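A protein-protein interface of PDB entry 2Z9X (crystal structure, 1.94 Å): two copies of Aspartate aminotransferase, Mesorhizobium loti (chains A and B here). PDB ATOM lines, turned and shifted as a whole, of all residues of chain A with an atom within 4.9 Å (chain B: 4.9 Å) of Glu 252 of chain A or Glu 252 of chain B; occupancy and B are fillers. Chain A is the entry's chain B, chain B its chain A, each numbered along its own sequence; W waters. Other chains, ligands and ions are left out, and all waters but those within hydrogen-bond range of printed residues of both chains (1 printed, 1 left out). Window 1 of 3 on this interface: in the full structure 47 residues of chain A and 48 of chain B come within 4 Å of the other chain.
The side-chain carboxylate (OE2) of Glu 252 of chain B sits close to the side-chain carboxylate (OE2) of Glu 252 of chain A, at 2.2 Å.
The backbone carbonyl oxygen of Val 250 of chain B sits close to the side-chain amide oxygen of Asn 254 of chain B, 3.4 Å away.
Among the printed residues, merely in contact across the chains: Leu 28 of chain A with Leu 28 of chain B (3.4 Å), Leu 28 of chain A with Ser 251 of chain B (3.8 Å), Pro 201 of chain A with Ser 251 of chain B (3.3 Å), Pro 202 of chain A with Val 250 of chain B (3.7 Å), Ser 249 of chain A with Gly 203 of chain B (3.9 Å), Ser 251 of chain A with Leu 28 of chain B (3.8 Å) and Ser 251 of chain A with Pro 201 of chain B (3.0 Å).
Of chain A, only Glu 252 comes within 4 Å of Glu 252 of chain B. Of the printed residues of chain B, Ser 249 of chain A touches Gly 203 (3.9 Å). Of the printed residues of chain A, Gly 203 of chain B touches Ser 249 (3.9 Å). Of the printed residues of chain A, Ser 251 of chain B touches Leu 28 (3.8 Å) and Pro 201 (3.3 Å). The nearest residue of chain B that does not touch Glu 252 of chain A is Ser 251 of chain B (4.4 Å). The nearest residue of chain A that does not touch Glu 252 of chain B is Ser 251 of chain A (4.2 Å).
Printed residues of chain A that touch a printed residue of chain B: Leu 28, Pro 201, Pro 202, Ser 249, Ser 251 and Glu 252. Of the 13 printed residues of chain B, 6 touch a printed residue of chain A. Printed residues of chain B that touch a printed residue of chain A: Leu 28, Pro 201, Gly 203, Val 250, Ser 251 and Glu 252. Among the printed residues, no Asp or Glu carboxylate lies within 4 Å of a Lys or Arg side-chain nitrogen of the other chain.
Leu 28 of chain B touches its own counterpart, Leu 28 of chain A. Leu 28 of chain A touches Ser 251 of chain B, and with the chains exchanged Ser 251 of chain A touches Leu 28 of chain B. Pro 202 of chain A touches Val 250 of chain B, but with the chains exchanged Val 250 of chain A does not touch Pro 202 of chain B (4.1 Å). Ser 249 of chain A touches Gly 203 of chain B, but with the chains exchanged Gly 203 of chain A does not touch Ser 249 of chain B (4.01 Å).
Water W1 lies within hydrogen-bond range of O of Pro 202 of chain B (2.6 Å), OE2 of Glu 252 of chain B (2.9 Å), N of Ser 251 of chain A (3.1 Å) and N of Glu 252 of chain A (3.5 Å).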
ATOM      1  N   LEU A  28      -4.554 -20.426 -14.597  1.00  0.00           N
ATOM      2  CA  LEU A  28      -3.862 -21.170 -15.650  1.00  0.00           C
ATOM      3  C   LEU A  28      -4.712 -21.350 -16.923  1.00  0.00           C
ATOM      4  O   LEU A  28      -4.183 -21.452 -18.028  1.00  0.00           O
ATOM      5  CB  LEU A  28      -3.445 -22.547 -15.121  1.00  0.00           C
ATOM      6  CG  LEU A  28      -2.124 -22.632 -14.368  1.00  0.00           C
ATOM      7  CD1 LEU A  28      -1.958 -24.031 -13.756  1.00  0.00           C
ATOM      8  CD2 LEU A  28      -0.959 -22.295 -15.343  1.00  0.00           C
ATOM      9  N   PRO A 201       2.057 -22.980 -10.420  1.00  0.00           N
ATOM     10  CA  PRO A 201       2.555 -24.189 -11.052  1.00  0.00           C
ATOM     11  C   PRO A 201       4.065 -24.080 -11.405  1.00  0.00           C
ATOM     12  O   PRO A 201       4.616 -22.975 -11.455  1.00  0.00           O
ATOM     13  CB  PRO A 201       1.666 -24.324 -12.304  1.00  0.00           C
ATOM     14  CG  PRO A 201       1.227 -22.936 -12.615  1.00  0.00           C
ATOM     15  CD  PRO A 201       1.175 -22.192 -11.309  1.00  0.00           C
ATOM     16  N   PRO A 202       4.723 -25.223 -11.610  1.00  0.00           N
ATOM     17  CA  PRO A 202       6.135 -25.273 -11.929  1.00  0.00           C
ATOM     18  C   PRO A 202       6.433 -24.818 -13.357  1.00  0.00           C
ATOM     19  O   PRO A 202       5.580 -24.974 -14.267  1.00  0.00           O
ATOM     20  CB  PRO A 202       6.465 -26.754 -11.761  1.00  0.00           C
ATOM     21  CG  PRO A 202       5.203 -27.446 -11.966  1.00  0.00           C
ATOM     22  CD  PRO A 202       4.123 -26.565 -11.543  1.00  0.00           C
ATOM     23  N   GLY A 203       7.622 -24.263 -13.552  1.00  0.00           N
ATOM     24  CA  GLY A 203       8.113 -23.998 -14.912  1.00  0.00           C
ATOM     25  C   GLY A 203       8.669 -22.602 -15.124  1.00  0.00           C
ATOM     26  O   GLY A 203       9.092 -22.282 -16.239  1.00  0.00           O
ATOM     27  N   LEU A 204       8.650 -21.767 -14.072  1.00  0.00           N
ATOM     28  CA  LEU A 204       9.313 -20.453 -14.101  1.00  0.00           C
ATOM     29  C   LEU A 204      10.357 -20.246 -12.996  1.00  0.00           C
ATOM     30  O   LEU A 204      10.395 -20.976 -11.994  1.00  0.00           O
ATOM     31  CB  LEU A 204       8.298 -19.307 -14.008  1.00  0.00           C
ATOM     32  CG  LEU A 204       7.163 -19.211 -15.024  1.00  0.00           C
ATOM     33  CD1 LEU A 204       6.190 -18.159 -14.524  1.00  0.00           C
ATOM     34  CD2 LEU A 204       7.671 -18.874 -16.436  1.00  0.00           C
ATOM     35  N   SER A 249       6.357 -18.302 -21.225  1.00  0.00           N
ATOM     36  CA  SER A 249       5.376 -19.311 -20.872  1.00  0.00           C
ATOM     37  C   SER A 249       4.085 -18.654 -20.409  1.00  0.00           C
ATOM     38  O   SER A 249       3.846 -18.483 -19.202  1.00  0.00           O
ATOM     39  CB  SER A 249       5.944 -20.277 -19.818  1.00  0.00           C
ATOM     40  OG  SER A 249       7.023 -21.009 -20.394  1.00  0.00           O
ATOM     41  N   VAL A 250       3.263 -18.277 -21.390  1.00  0.00           N
ATOM     42  CA  VAL A 250       2.084 -17.426 -21.166  1.00  0.00           C
ATOM     43  C   VAL A 250       1.172 -17.932 -20.067  1.00  0.00           C
ATOM     44  O   VAL A 250       0.783 -17.163 -19.204  1.00  0.00           O
ATOM     45  CB  VAL A 250       1.277 -17.153 -22.486  1.00  0.00           C
ATOM     46  CG1 VAL A 250      -0.046 -16.418 -22.177  1.00  0.00           C
ATOM     47  CG2 VAL A 250       2.140 -16.315 -23.462  1.00  0.00           C
ATOM     48  N   SER A 251       0.823 -19.215 -20.103  1.00  0.00           N
ATOM     49  CA  SER A 251      -0.078 -19.765 -19.079  1.00  0.00           C
ATOM     50  C   SER A 251       0.525 -19.743 -17.689  1.00  0.00           C
ATOM     51  O   SER A 251      -0.192 -19.464 -16.722  1.00  0.00           O
ATOM     52  CB  SER A 251      -0.495 -21.195 -19.415  1.00  0.00           C
ATOM     53  OG  SER A 251      -1.207 -21.161 -20.640  1.00  0.00           O
ATOM     54  N   GLU A 252       1.817 -20.034 -17.582  1.00  0.00           N
ATOM     55  CA  GLU A 252       2.508 -19.983 -16.298  1.00  0.00           C
ATOM     56  C   GLU A 252       2.522 -18.565 -15.738  1.00  0.00           C
ATOM     57  O   GLU A 252       2.364 -18.360 -14.534  1.00  0.00           O
ATOM     58  CB  GLU A 252       3.938 -20.508 -16.439  1.00  0.00           C
ATOM     59  CG  GLU A 252       4.041 -21.857 -17.131  1.00  0.00           C
ATOM     60  CD  GLU A 252       3.388 -22.971 -16.335  1.00  0.00           C
ATOM     61  OE1 GLU A 252       3.410 -22.902 -15.089  1.00  0.00           O
ATOM     62  OE2 GLU A 252       2.855 -23.914 -16.957  1.00  0.00           O
ATOM     63  N   ILE A 253       2.712 -17.590 -16.620  1.00  0.00           N
ATOM     64  CA  ILE A 253       2.641 -16.159 -16.237  1.00  0.00           C
ATOM     65  C   ILE A 253       1.242 -15.782 -15.711  1.00  0.00           C
ATOM     66  O   ILE A 253       1.120 -15.045 -14.720  1.00  0.00           O
ATOM     67  CB  ILE A 253       3.036 -15.225 -17.407  1.00  0.00           C
ATOM     68  CG1 ILE A 253       4.548 -15.310 -17.699  1.00  0.00           C
ATOM     69  CG2 ILE A 253       2.615 -13.782 -17.113  1.00  0.00           C
ATOM     70  CD1 ILE A 253       5.442 -14.772 -16.582  1.00  0.00           C
ATOM     71  N   ASN A 254       0.190 -16.287 -16.369  1.00  0.00           N
ATOM     72  CA  ASN A 254      -1.203 -16.117 -15.876  1.00  0.00           C
ATOM     73  C   ASN A 254      -1.380 -16.673 -14.481  1.00  0.00           C
ATOM     74  O   ASN A 254      -2.022 -16.051 -13.637  1.00  0.00           O
ATOM     75  CB  ASN A 254      -2.209 -16.827 -16.821  1.00  0.00           C
ATOM     76  CG  ASN A 254      -2.451 -16.062 -18.117  1.00  0.00           C
ATOM     77  OD1 ASN A 254      -2.606 -16.658 -19.204  1.00  0.00           O
ATOM     78  ND2 ASN A 254      -2.480 -14.746 -18.017  1.00  0.00           N
ATOM     79  N   GLY A 255      -0.830 -17.859 -14.235  1.00  0.00           N
ATOM     80  CA  GLY A 255      -0.883 -18.473 -12.914  1.00  0.00           C
ATOM     81  C   GLY A 255      -0.079 -17.710 -11.865  1.00  0.00           C
ATOM     82  O   GLY A 255      -0.507 -17.554 -10.711  1.00  0.00           O
ATOM     83  N   LEU A 256       1.101 -17.242 -12.261  1.00  0.00           N
ATOM     84  CA  LEU A 256       1.939 -16.490 -11.349  1.00  0.00           C
ATOM     85  C   LEU A 256       1.291 -15.159 -10.967  1.00  0.00           C
ATOM     86  O   LEU A 256       1.448 -14.711  -9.837  1.00  0.00           O
ATOM     87  CB  LEU A 256       3.336 -16.260 -11.944  1.00  0.00           C
ATOM     88  CG  LEU A 256       4.338 -15.509 -11.048  1.00  0.00           C
ATOM     89  CD1 LEU A 256       4.567 -16.217  -9.681  1.00  0.00           C
ATOM     90  CD2 LEU A 256       5.650 -15.297 -11.781  1.00  0.00           C
ATOM     91  N   LEU B  28      -4.997 -27.860 -17.963  1.00  0.00           N
ATOM     92  CA  LEU B  28      -3.958 -27.154 -17.192  1.00  0.00           C
ATOM     93  C   LEU B  28      -4.338 -26.960 -15.732  1.00  0.00           C
ATOM     94  O   LEU B  28      -3.460 -26.821 -14.877  1.00  0.00           O
ATOM     95  CB  LEU B  28      -3.721 -25.765 -17.777  1.00  0.00           C
ATOM     96  CG  LEU B  28      -3.086 -25.702 -19.150  1.00  0.00           C
ATOM     97  CD1 LEU B  28      -3.112 -24.266 -19.616  1.00  0.00           C
ATOM     98  CD2 LEU B  28      -1.669 -26.205 -19.016  1.00  0.00           C
ATOM     99  N   PRO B 201      -0.586 -24.733 -24.411  1.00  0.00           N
ATOM    100  CA  PRO B 201       0.131 -23.473 -24.146  1.00  0.00           C
ATOM    101  C   PRO B 201       1.648 -23.607 -24.362  1.00  0.00           C
ATOM    102  O   PRO B 201       2.145 -24.722 -24.500  1.00  0.00           O
ATOM    103  CB  PRO B 201      -0.193 -23.163 -22.672  1.00  0.00           C
ATOM    104  CG  PRO B 201      -0.827 -24.390 -22.124  1.00  0.00           C
ATOM    105  CD  PRO B 201      -0.992 -25.421 -23.173  1.00  0.00           C
ATOM    106  N   PRO B 202       2.377 -22.477 -24.389  1.00  0.00           N
ATOM    107  CA  PRO B 202       3.791 -22.630 -24.667  1.00  0.00           C
ATOM    108  C   PRO B 202       4.521 -23.178 -23.453  1.00  0.00           C
ATOM    109  O   PRO B 202       4.092 -22.953 -22.323  1.00  0.00           O
ATOM    110  CB  PRO B 202       4.269 -21.198 -24.959  1.00  0.00           C
ATOM    111  CG  PRO B 202       3.065 -20.318 -24.924  1.00  0.00           C
ATOM    112  CD  PRO B 202       2.004 -21.069 -24.165  1.00  0.00           C
ATOM    113  N   GLY B 203       5.630 -23.866 -23.684  1.00  0.00           N
ATOM    114  CA  GLY B 203       6.500 -24.221 -22.588  1.00  0.00           C
ATOM    115  C   GLY B 203       7.136 -25.577 -22.700  1.00  0.00           C
ATOM    116  O   GLY B 203       8.002 -25.904 -21.881  1.00  0.00           O
ATOM    117  N   LEU B 204       6.734 -26.367 -23.704  1.00  0.00           N
ATOM    118  CA  LEU B 204       7.357 -27.689 -23.894  1.00  0.00           C
ATOM    119  C   LEU B 204       7.935 -27.879 -25.287  1.00  0.00           C
ATOM    120  O   LEU B 204       7.564 -27.162 -26.226  1.00  0.00           O
ATOM    121  CB  LEU B 204       6.374 -28.807 -23.607  1.00  0.00           C
ATOM    122  CG  LEU B 204       5.753 -28.915 -22.218  1.00  0.00           C
ATOM    123  CD1 LEU B 204       4.767 -30.084 -22.269  1.00  0.00           C
ATOM    124  CD2 LEU B 204       6.809 -29.169 -21.127  1.00  0.00           C
ATOM    125  N   SER B 249       7.535 -29.807 -16.087  1.00  0.00           N
ATOM    126  CA  SER B 249       6.491 -28.798 -16.022  1.00  0.00           C
ATOM    127  C   SER B 249       5.143 -29.497 -15.959  1.00  0.00           C
ATOM    128  O   SER B 249       4.465 -29.691 -16.985  1.00  0.00           O
ATOM    129  CB  SER B 249       6.575 -27.844 -17.227  1.00  0.00           C
ATOM    130  OG  SER B 249       7.856 -27.232 -17.266  1.00  0.00           O
ATOM    131  N   VAL B 250       4.767 -29.874 -14.742  1.00  0.00           N
ATOM    132  CA  VAL B 250       3.615 -30.737 -14.498  1.00  0.00           C
ATOM    133  C   VAL B 250       2.338 -30.253 -15.180  1.00  0.00           C
ATOM    134  O   VAL B 250       1.616 -31.038 -15.811  1.00  0.00           O
ATOM    135  CB  VAL B 250       3.400 -30.976 -12.971  1.00  0.00           C
ATOM    136  CG1 VAL B 250       2.090 -31.730 -12.728  1.00  0.00           C
ATOM    137  CG2 VAL B 250       4.597 -31.748 -12.369  1.00  0.00           C
ATOM    138  N   SER B 251       2.015 -28.973 -15.015  1.00  0.00           N
ATOM    139  CA  SER B 251       0.758 -28.464 -15.548  1.00  0.00           C
ATOM    140  C   SER B 251       0.772 -28.486 -17.092  1.00  0.00           C
ATOM    141  O   SER B 251      -0.232 -28.829 -17.702  1.00  0.00           O
ATOM    142  CB  SER B 251       0.452 -27.058 -15.028  1.00  0.00           C
ATOM    143  OG  SER B 251       0.321 -27.060 -13.616  1.00  0.00           O
ATOM    144  N   GLU B 252       1.894 -28.124 -17.694  1.00  0.00           N
ATOM    145  CA  GLU B 252       2.051 -28.209 -19.137  1.00  0.00           C
ATOM    146  C   GLU B 252       1.893 -29.644 -19.679  1.00  0.00           C
ATOM    147  O   GLU B 252       1.389 -29.874 -20.716  1.00  0.00           O
ATOM    148  CB  GLU B 252       3.337 -27.564 -19.653  1.00  0.00           C
ATOM    149  CG  GLU B 252       3.607 -26.164 -19.204  1.00  0.00           C
ATOM    150  CD  GLU B 252       2.659 -25.193 -19.764  1.00  0.00           C
ATOM    151  OE1 GLU B 252       2.159 -25.442 -20.850  1.00  0.00           O
ATOM    152  OE2 GLU B 252       2.385 -24.176 -19.132  1.00  0.00           O
ATOM    153  N   ILE B 253       2.395 -30.588 -18.930  1.00  0.00           N
ATOM    154  CA  ILE B 253       2.230 -31.999 -19.296  1.00  0.00           C
ATOM    155  C   ILE B 253       0.736 -32.378 -19.243  1.00  0.00           C
ATOM    156  O   ILE B 253       0.228 -33.116 -20.112  1.00  0.00           O
ATOM    157  CB  ILE B 253       3.096 -32.930 -18.397  1.00  0.00           C
ATOM    158  CG1 ILE B 253       4.598 -32.830 -18.753  1.00  0.00           C
ATOM    159  CG2 ILE B 253       2.625 -34.387 -18.472  1.00  0.00           C
ATOM    160  CD1 ILE B 253       5.004 -33.364 -20.168  1.00  0.00           C
ATOM    161  N   ASN B 254       0.025 -31.867 -18.237  1.00  0.00           N
ATOM    162  CA  ASN B 254      -1.424 -32.042 -18.162  1.00  0.00           C
ATOM    163  C   ASN B 254      -2.126 -31.492 -19.401  1.00  0.00           C
ATOM    164  O   ASN B 254      -3.028 -32.138 -19.940  1.00  0.00           O
ATOM    165  CB  ASN B 254      -2.014 -31.398 -16.893  1.00  0.00           C
ATOM    166  CG  ASN B 254      -1.729 -32.210 -15.608  1.00  0.00           C
ATOM    167  OD1 ASN B 254      -1.518 -31.633 -14.541  1.00  0.00           O
ATOM    168  ND2 ASN B 254      -1.733 -33.524 -15.706  1.00  0.00           N
ATOM    169  N   GLY B 255      -1.737 -30.291 -19.840  1.00  0.00           N
ATOM    170  CA  GLY B 255      -2.313 -29.712 -21.058  1.00  0.00           C
ATOM    171  C   GLY B 255      -1.968 -30.504 -22.309  1.00  0.00           C
ATOM    172  O   GLY B 255      -2.815 -30.688 -23.197  1.00  0.00           O
ATOM    173  N   LEU B 256      -0.720 -30.957 -22.390  1.00  0.00           N
ATOM    174  CA  LEU B 256      -0.270 -31.743 -23.536  1.00  0.00           C
ATOM    175  C   LEU B 256      -0.998 -33.081 -23.674  1.00  0.00           C
ATOM    176  O   LEU B 256      -1.330 -33.509 -24.775  1.00  0.00           O
ATOM    177  CB  LEU B 256       1.258 -31.955 -23.468  1.00  0.00           C
ATOM    178  CG  LEU B 256       1.855 -32.698 -24.672  1.00  0.00           C
ATOM    179  CD1 LEU B 256       1.623 -31.923 -25.959  1.00  0.00           C
ATOM    180  CD2 LEU B 256       3.339 -32.977 -24.441  1.00  0.00           C
HETATM  181  O   HOH W   1       2.653 -21.673 -20.553  1.00  0.00           O
